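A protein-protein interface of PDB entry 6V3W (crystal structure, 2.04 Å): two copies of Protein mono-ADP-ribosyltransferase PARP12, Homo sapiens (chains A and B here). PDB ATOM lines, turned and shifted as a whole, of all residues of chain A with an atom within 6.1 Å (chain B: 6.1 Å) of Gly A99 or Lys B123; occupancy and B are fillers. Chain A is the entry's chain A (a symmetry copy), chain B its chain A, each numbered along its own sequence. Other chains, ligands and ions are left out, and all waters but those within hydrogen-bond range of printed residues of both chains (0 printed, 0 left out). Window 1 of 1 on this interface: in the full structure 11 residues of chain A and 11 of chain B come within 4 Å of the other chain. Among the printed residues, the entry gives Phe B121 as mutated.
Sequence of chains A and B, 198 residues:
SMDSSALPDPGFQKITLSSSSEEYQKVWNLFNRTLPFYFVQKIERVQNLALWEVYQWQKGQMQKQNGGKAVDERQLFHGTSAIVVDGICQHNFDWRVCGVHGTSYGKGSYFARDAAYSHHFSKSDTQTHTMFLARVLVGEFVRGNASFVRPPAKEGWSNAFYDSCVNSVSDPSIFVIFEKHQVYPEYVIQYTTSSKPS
Of the 15 printed residues of chain B, 4 touch a printed residue of chain A. Printed residues of chain B that touch a printed residue of chain A: Ser B81, Cys B98, Lys B123 and Asp B125. Along chain A the printed residues that touch a printed residue of chain B span positions 96 to 99. Among the printed residues, 5 pairs touch across the chains. Among the printed residues, Asp or Glu carboxylates within 4 Å of a Lys or Arg side-chain nitrogen of the other chain: Arg A96 with Asp B125 (3.2 Å).
Cys A98 touches its own counterpart, Cys B98. Of the 5 pairs that touch across the chains among the printed residues, 1 has its exchanged pair printed and touching as well.
Lys B123 touches Arg A96 (CD to O, 3.6 Å). Gly A99 touches Lys B123.
Of chain B, only Lys B123 comes within 4 Å of Gly A99. Lys B123 touches two residues of chain A. Of the printed residues of chain B, Arg A96 touches Ser B81 (3.5 Å), Lys B123 (3.6 Å) and Asp B125 (3.2 Å). Of the printed residues of chain B, Cys A98 touches Cys B98 (2.0 Å). Of the printed residues of chain A, Ser B81 touches Arg A96 (3.5 Å). Trp A95 touches none of the printed residues of chain B. Thr B130 touches none of the printed residues of chain A. The nearest residue of chain B that does not touch Gly A99 is Cys B98 (5.6 Å). The nearest residue of chain A that does not touch Lys B123 is Trp A95 (4.5 Å). The nearest printed residue of chain B that does not touch Cys A98 is Lys B123 (4.9 Å).
The side-chain hydroxyl (OG) of Ser B81 sits at hydrogen-bond distance from the backbone carbonyl oxygen (O) of Arg A96. SG of Cys B98 forms a disulfide with SG of Cys A98, at 2.0 Å. The side-chain carboxylate of Asp B125 is in salt-bridge range of the guanidinium group of Arg A96, at 3.2 Å.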
ATOM      1  N   TRP A  95     -24.913  26.372  22.230  1.00  0.00           N
ATOM      2  CA  TRP A  95     -24.042  27.560  22.431  1.00  0.00           C
ATOM      3  C   TRP A  95     -22.882  27.568  21.427  1.00  0.00           C
ATOM      4  O   TRP A  95     -22.282  28.633  21.260  1.00  0.00           O
ATOM      5  CB  TRP A  95     -23.506  27.587  23.860  1.00  0.00           C
ATOM      6  CG  TRP A  95     -22.495  26.513  24.118  1.00  0.00           C
ATOM      7  CD1 TRP A  95     -22.737  25.251  24.581  1.00  0.00           C
ATOM      8  CD2 TRP A  95     -21.077  26.602  23.904  1.00  0.00           C
ATOM      9  NE1 TRP A  95     -21.566  24.548  24.672  1.00  0.00           N
ATOM     10  CE2 TRP A  95     -20.531  25.351  24.264  1.00  0.00           C
ATOM     11  CE3 TRP A  95     -20.221  27.612  23.444  1.00  0.00           C
ATOM     12  CZ2 TRP A  95     -19.163  25.095  24.195  1.00  0.00           C
ATOM     13  CZ3 TRP A  95     -18.869  27.357  23.366  1.00  0.00           C
ATOM     14  CH2 TRP A  95     -18.352  26.114  23.741  1.00  0.00           C
ATOM     15  N   ARG A  96     -22.560  26.432  20.804  1.00  0.00           N
ATOM     16  CA  ARG A  96     -21.389  26.308  19.888  1.00  0.00           C
ATOM     17  C   ARG A  96     -21.666  27.007  18.556  1.00  0.00           C
ATOM     18  O   ARG A  96     -20.698  27.239  17.811  1.00  0.00           O
ATOM     19  CB  ARG A  96     -21.025  24.843  19.647  1.00  0.00           C
ATOM     20  CG  ARG A  96     -20.019  24.317  20.656  1.00  0.00           C
ATOM     21  CD  ARG A  96     -19.927  22.809  20.617  1.00  0.00           C
ATOM     22  NE  ARG A  96     -20.739  22.213  21.668  1.00  0.00           N
ATOM     23  CZ  ARG A  96     -21.487  21.122  21.536  1.00  0.00           C
ATOM     24  NH1 ARG A  96     -22.162  20.669  22.579  1.00  0.00           N
ATOM     25  NH2 ARG A  96     -21.564  20.487  20.377  1.00  0.00           N
ATOM     26  N   VAL A  97     -22.931  27.323  18.268  1.00  0.00           N
ATOM     27  CA  VAL A  97     -23.313  28.114  17.063  1.00  0.00           C
ATOM     28  C   VAL A  97     -22.607  29.470  17.140  1.00  0.00           C
ATOM     29  O   VAL A  97     -22.017  29.857  16.131  1.00  0.00           O
ATOM     30  CB  VAL A  97     -24.837  28.288  16.914  1.00  0.00           C
ATOM     31  CG1 VAL A  97     -25.188  29.281  15.813  1.00  0.00           C
ATOM     32  CG2 VAL A  97     -25.528  26.958  16.670  1.00  0.00           C
ATOM     33  N   CYS A  98     -22.664  30.153  18.288  1.00  0.00           N
ATOM     34  CA  CYS A  98     -22.194  31.556  18.444  1.00  0.00           C
ATOM     35  C   CYS A  98     -20.864  31.647  19.198  1.00  0.00           C
ATOM     36  O   CYS A  98     -20.068  32.534  18.852  1.00  0.00           O
ATOM     37  CB  CYS A  98     -23.226  32.401  19.179  1.00  0.00           C
ATOM     38  SG  CYS A  98     -24.681  32.808  18.181  1.00  0.00           S
ATOM     39  N   GLY A  99     -20.641  30.792  20.199  1.00  0.00           N
ATOM     40  CA  GLY A  99     -19.672  31.040  21.286  1.00  0.00           C
ATOM     41  C   GLY A  99     -20.152  32.136  22.236  1.00  0.00           C
ATOM     42  O   GLY A  99     -21.283  32.649  22.056  1.00  0.00           O
ATOM     43  N   VAL A 100     -19.325  32.465  23.232  1.00  0.00           N
ATOM     44  CA  VAL A 100     -19.538  33.536  24.255  1.00  0.00           C
ATOM     45  C   VAL A 100     -18.253  34.379  24.311  1.00  0.00           C
ATOM     46  O   VAL A 100     -17.171  33.767  24.388  1.00  0.00           O
ATOM     47  CB  VAL A 100     -19.865  32.929  25.639  1.00  0.00           C
ATOM     48  CG1 VAL A 100     -20.258  33.996  26.655  1.00  0.00           C
ATOM     49  CG2 VAL A 100     -20.934  31.844  25.558  1.00  0.00           C
ATOM     50  N   HIS A 101     -18.349  35.713  24.271  1.00  0.00           N
ATOM     51  CA  HIS A 101     -17.170  36.626  24.333  1.00  0.00           C
ATOM     52  C   HIS A 101     -17.564  38.004  24.882  1.00  0.00           C
ATOM     53  O   HIS A 101     -18.773  38.274  24.943  1.00  0.00           O
ATOM     54  CB  HIS A 101     -16.479  36.722  22.958  1.00  0.00           C
ATOM     55  CG  HIS A 101     -15.286  35.830  22.802  1.00  0.00           C
ATOM     56  ND1 HIS A 101     -15.386  34.444  22.742  1.00  0.00           N
ATOM     57  CD2 HIS A 101     -13.970  36.114  22.674  1.00  0.00           C
ATOM     58  CE1 HIS A 101     -14.186  33.918  22.593  1.00  0.00           C
ATOM     59  NE2 HIS A 101     -13.297  34.921  22.545  1.00  0.00           N
ATOM     60  N   GLY B  79     -16.415  29.741   8.037  1.00  0.00           N
ATOM     61  CA  GLY B  79     -16.482  28.515   8.855  1.00  0.00           C
ATOM     62  C   GLY B  79     -17.684  28.540   9.788  1.00  0.00           C
ATOM     63  O   GLY B  79     -17.873  29.580  10.440  1.00  0.00           O
ATOM     64  N   THR B  80     -18.479  27.461   9.827  1.00  0.00           N
ATOM     65  CA  THR B  80     -19.726  27.349  10.644  1.00  0.00           C
ATOM     66  C   THR B  80     -19.729  26.020  11.385  1.00  0.00           C
ATOM     67  O   THR B  80     -18.779  25.271  11.219  1.00  0.00           O
ATOM     68  CB  THR B  80     -21.007  27.391   9.795  1.00  0.00           C
ATOM     69  OG1 THR B  80     -20.836  26.602   8.619  1.00  0.00           O
ATOM     70  CG2 THR B  80     -21.391  28.787   9.377  1.00  0.00           C
ATOM     71  N   SER B  81     -20.769  25.776  12.179  1.00  0.00           N
ATOM     72  CA  SER B  81     -21.159  24.450  12.709  1.00  0.00           C
ATOM     73  C   SER B  81     -22.107  23.829  11.707  1.00  0.00           C
ATOM     74  O   SER B  81     -22.882  24.587  11.054  1.00  0.00           O
ATOM     75  CB  SER B  81     -21.843  24.563  14.022  1.00  0.00           C
ATOM     76  OG  SER B  81     -21.132  25.461  14.845  1.00  0.00           O
ATOM     77  N   ALA B  82     -22.058  22.510  11.610  1.00  0.00           N
ATOM     78  CA  ALA B  82     -22.927  21.700  10.731  1.00  0.00           C
ATOM     79  C   ALA B  82     -24.393  22.047  11.011  1.00  0.00           C
ATOM     80  O   ALA B  82     -25.217  21.979  10.088  1.00  0.00           O
ATOM     81  CB  ALA B  82     -22.658  20.233  10.999  1.00  0.00           C
ATOM     82  N   CYS B  98     -25.938  36.097  16.309  1.00  0.00           N
ATOM     83  CA  CYS B  98     -24.891  35.928  17.353  1.00  0.00           C
ATOM     84  C   CYS B  98     -24.473  37.262  17.983  1.00  0.00           C
ATOM     85  O   CYS B  98     -24.182  37.259  19.188  1.00  0.00           O
ATOM     86  CB  CYS B  98     -23.651  35.253  16.783  1.00  0.00           C
ATOM     87  SG  CYS B  98     -23.868  33.485  16.458  1.00  0.00           S
ATOM     88  N   HIS B 119     -11.153  28.330   9.160  1.00  0.00           N
ATOM     89  CA  HIS B 119     -11.084  27.027   9.879  1.00  0.00           C
ATOM     90  C   HIS B 119     -11.216  27.193  11.408  1.00  0.00           C
ATOM     91  O   HIS B 119     -11.833  26.317  12.037  1.00  0.00           O
ATOM     92  CB  HIS B 119      -9.820  26.262   9.522  1.00  0.00           C
ATOM     93  CG  HIS B 119      -9.669  25.021  10.334  1.00  0.00           C
ATOM     94  ND1 HIS B 119     -10.578  23.979  10.252  1.00  0.00           N
ATOM     95  CD2 HIS B 119      -8.773  24.685  11.286  1.00  0.00           C
ATOM     96  CE1 HIS B 119     -10.243  23.049  11.124  1.00  0.00           C
ATOM     97  NE2 HIS B 119      -9.128  23.453  11.767  1.00  0.00           N
ATOM     98  N   HIS B 120     -10.653  28.249  11.993  1.00  0.00           N
ATOM     99  CA  HIS B 120     -10.736  28.533  13.452  1.00  0.00           C
ATOM    100  C   HIS B 120     -12.204  28.608  13.887  1.00  0.00           C
ATOM    101  O   HIS B 120     -12.444  28.399  15.087  1.00  0.00           O
ATOM    102  CB  HIS B 120      -9.985  29.818  13.869  1.00  0.00           C
ATOM    103  CG  HIS B 120      -8.550  29.889  13.449  1.00  0.00           C
ATOM    104  ND1 HIS B 120      -8.063  30.914  12.653  1.00  0.00           N
ATOM    105  CD2 HIS B 120      -7.492  29.087  13.711  1.00  0.00           C
ATOM    106  CE1 HIS B 120      -6.770  30.731  12.438  1.00  0.00           C
ATOM    107  NE2 HIS B 120      -6.400  29.621  13.070  1.00  0.00           N
ATOM    108  N   PHE B 121     -13.155  28.908  12.992  1.00  0.00           N
ATOM    109  CA  PHE B 121     -14.582  29.083  13.396  1.00  0.00           C
ATOM    110  C   PHE B 121     -15.446  27.885  12.959  1.00  0.00           C
ATOM    111  O   PHE B 121     -16.654  27.905  13.189  1.00  0.00           O
ATOM    112  CB  PHE B 121     -15.109  30.416  12.865  1.00  0.00           C
ATOM    113  CG  PHE B 121     -14.243  31.596  13.234  1.00  0.00           C
ATOM    114  CD1 PHE B 121     -13.187  31.991  12.415  1.00  0.00           C
ATOM    115  CD2 PHE B 121     -14.470  32.309  14.396  1.00  0.00           C
ATOM    116  CE1 PHE B 121     -12.392  33.077  12.743  1.00  0.00           C
ATOM    117  CE2 PHE B 121     -13.670  33.394  14.725  1.00  0.00           C
ATOM    118  CZ  PHE B 121     -12.630  33.771  13.904  1.00  0.00           C
ATOM    119  N   SER B 122     -14.855  26.838  12.390  1.00  0.00           N
ATOM    120  CA  SER B 122     -15.552  25.575  12.040  1.00  0.00           C
ATOM    121  C   SER B 122     -15.485  24.609  13.227  1.00  0.00           C
ATOM    122  O   SER B 122     -14.636  23.738  13.202  1.00  0.00           O
ATOM    123  CB  SER B 122     -14.954  24.952  10.810  1.00  0.00           C
ATOM    124  OG  SER B 122     -15.036  25.841   9.695  1.00  0.00           O
ATOM    125  N   LYS B 123     -16.390  24.739  14.194  1.00  0.00           N
ATOM    126  CA  LYS B 123     -16.443  23.896  15.422  1.00  0.00           C
ATOM    127  C   LYS B 123     -17.091  22.530  15.098  1.00  0.00           C
ATOM    128  O   LYS B 123     -18.030  22.487  14.256  1.00  0.00           O
ATOM    129  CB  LYS B 123     -17.170  24.716  16.491  1.00  0.00           C
ATOM    130  CG  LYS B 123     -16.703  26.166  16.614  1.00  0.00           C
ATOM    131  CD  LYS B 123     -17.094  26.784  17.950  1.00  0.00           C
ATOM    132  CE  LYS B 123     -16.606  28.203  18.159  1.00  0.00           C
ATOM    133  NZ  LYS B 123     -17.002  28.699  19.500  1.00  0.00           N
ATOM    134  N   SER B 124     -16.633  21.428  15.709  1.00  0.00           N
ATOM    135  CA  SER B 124     -17.193  20.086  15.394  1.00  0.00           C
ATOM    136  C   SER B 124     -17.419  19.130  16.587  1.00  0.00           C
ATOM    137  O   SER B 124     -18.464  18.417  16.561  1.00  0.00           O
ATOM    138  CB  SER B 124     -16.351  19.432  14.374  1.00  0.00           C
ATOM    139  OG  SER B 124     -17.087  18.392  13.766  1.00  0.00           O
ATOM    140  N   ASP B 125     -16.477  18.984  17.523  1.00  0.00           N
ATOM    141  CA  ASP B 125     -16.457  17.825  18.471  1.00  0.00           C
ATOM    142  C   ASP B 125     -16.399  16.515  17.671  1.00  0.00           C
ATOM    143  O   ASP B 125     -16.769  15.473  18.218  1.00  0.00           O
ATOM    144  CB  ASP B 125     -17.718  17.687  19.340  1.00  0.00           C
ATOM    145  CG  ASP B 125     -18.072  18.861  20.233  1.00  0.00           C
ATOM    146  OD1 ASP B 125     -17.470  19.937  20.080  1.00  0.00           O
ATOM    147  OD2 ASP B 125     -18.965  18.679  21.081  1.00  0.00           O
ATOM    148  N   THR B 128     -15.146  15.720  11.202  1.00  0.00           N
ATOM    149  CA  THR B 128     -15.747  16.441  10.061  1.00  0.00           C
ATOM    150  C   THR B 128     -15.995  17.906  10.443  1.00  0.00           C
ATOM    151  O   THR B 128     -16.635  18.173  11.487  1.00  0.00           O
ATOM    152  CB  THR B 128     -16.986  15.703   9.559  1.00  0.00           C
ATOM    153  OG1 THR B 128     -16.451  14.403   9.353  1.00  0.00           O
ATOM    154  CG2 THR B 128     -17.569  16.264   8.280  1.00  0.00           C
ATOM    155  N   HIS B 129     -15.475  18.800   9.611  1.00  0.00           N
ATOM    156  CA  HIS B 129     -15.659  20.271   9.717  1.00  0.00           C
ATOM    157  C   HIS B 129     -16.425  20.770   8.497  1.00  0.00           C
ATOM    158  O   HIS B 129     -16.322  20.151   7.427  1.00  0.00           O
ATOM    159  CB  HIS B 129     -14.306  20.972   9.818  1.00  0.00           C
ATOM    160  CG  HIS B 129     -13.563  20.665  11.068  1.00  0.00           C
ATOM    161  ND1 HIS B 129     -13.598  21.504  12.169  1.00  0.00           N
ATOM    162  CD2 HIS B 129     -12.788  19.608  11.399  1.00  0.00           C
ATOM    163  CE1 HIS B 129     -12.866  20.976  13.133  1.00  0.00           C
ATOM    164  NE2 HIS B 129     -12.373  19.802  12.691  1.00  0.00           N
ATOM    165  N   THR B 130     -17.127  21.886   8.641  1.00  0.00           N
ATOM    166  CA  THR B 130     -17.917  22.464   7.534  1.00  0.00           C
ATOM    167  C   THR B 130     -17.564  23.928   7.352  1.00  0.00           C
ATOM    168  O   THR B 130     -17.421  24.646   8.380  1.00  0.00           O
ATOM    169  CB  THR B 130     -19.423  22.357   7.759  1.00  0.00           C
ATOM    170  OG1 THR B 130     -19.715  20.979   7.926  1.00  0.00           O
ATOM    171  CG2 THR B 130     -20.221  22.830   6.569  1.00  0.00           C
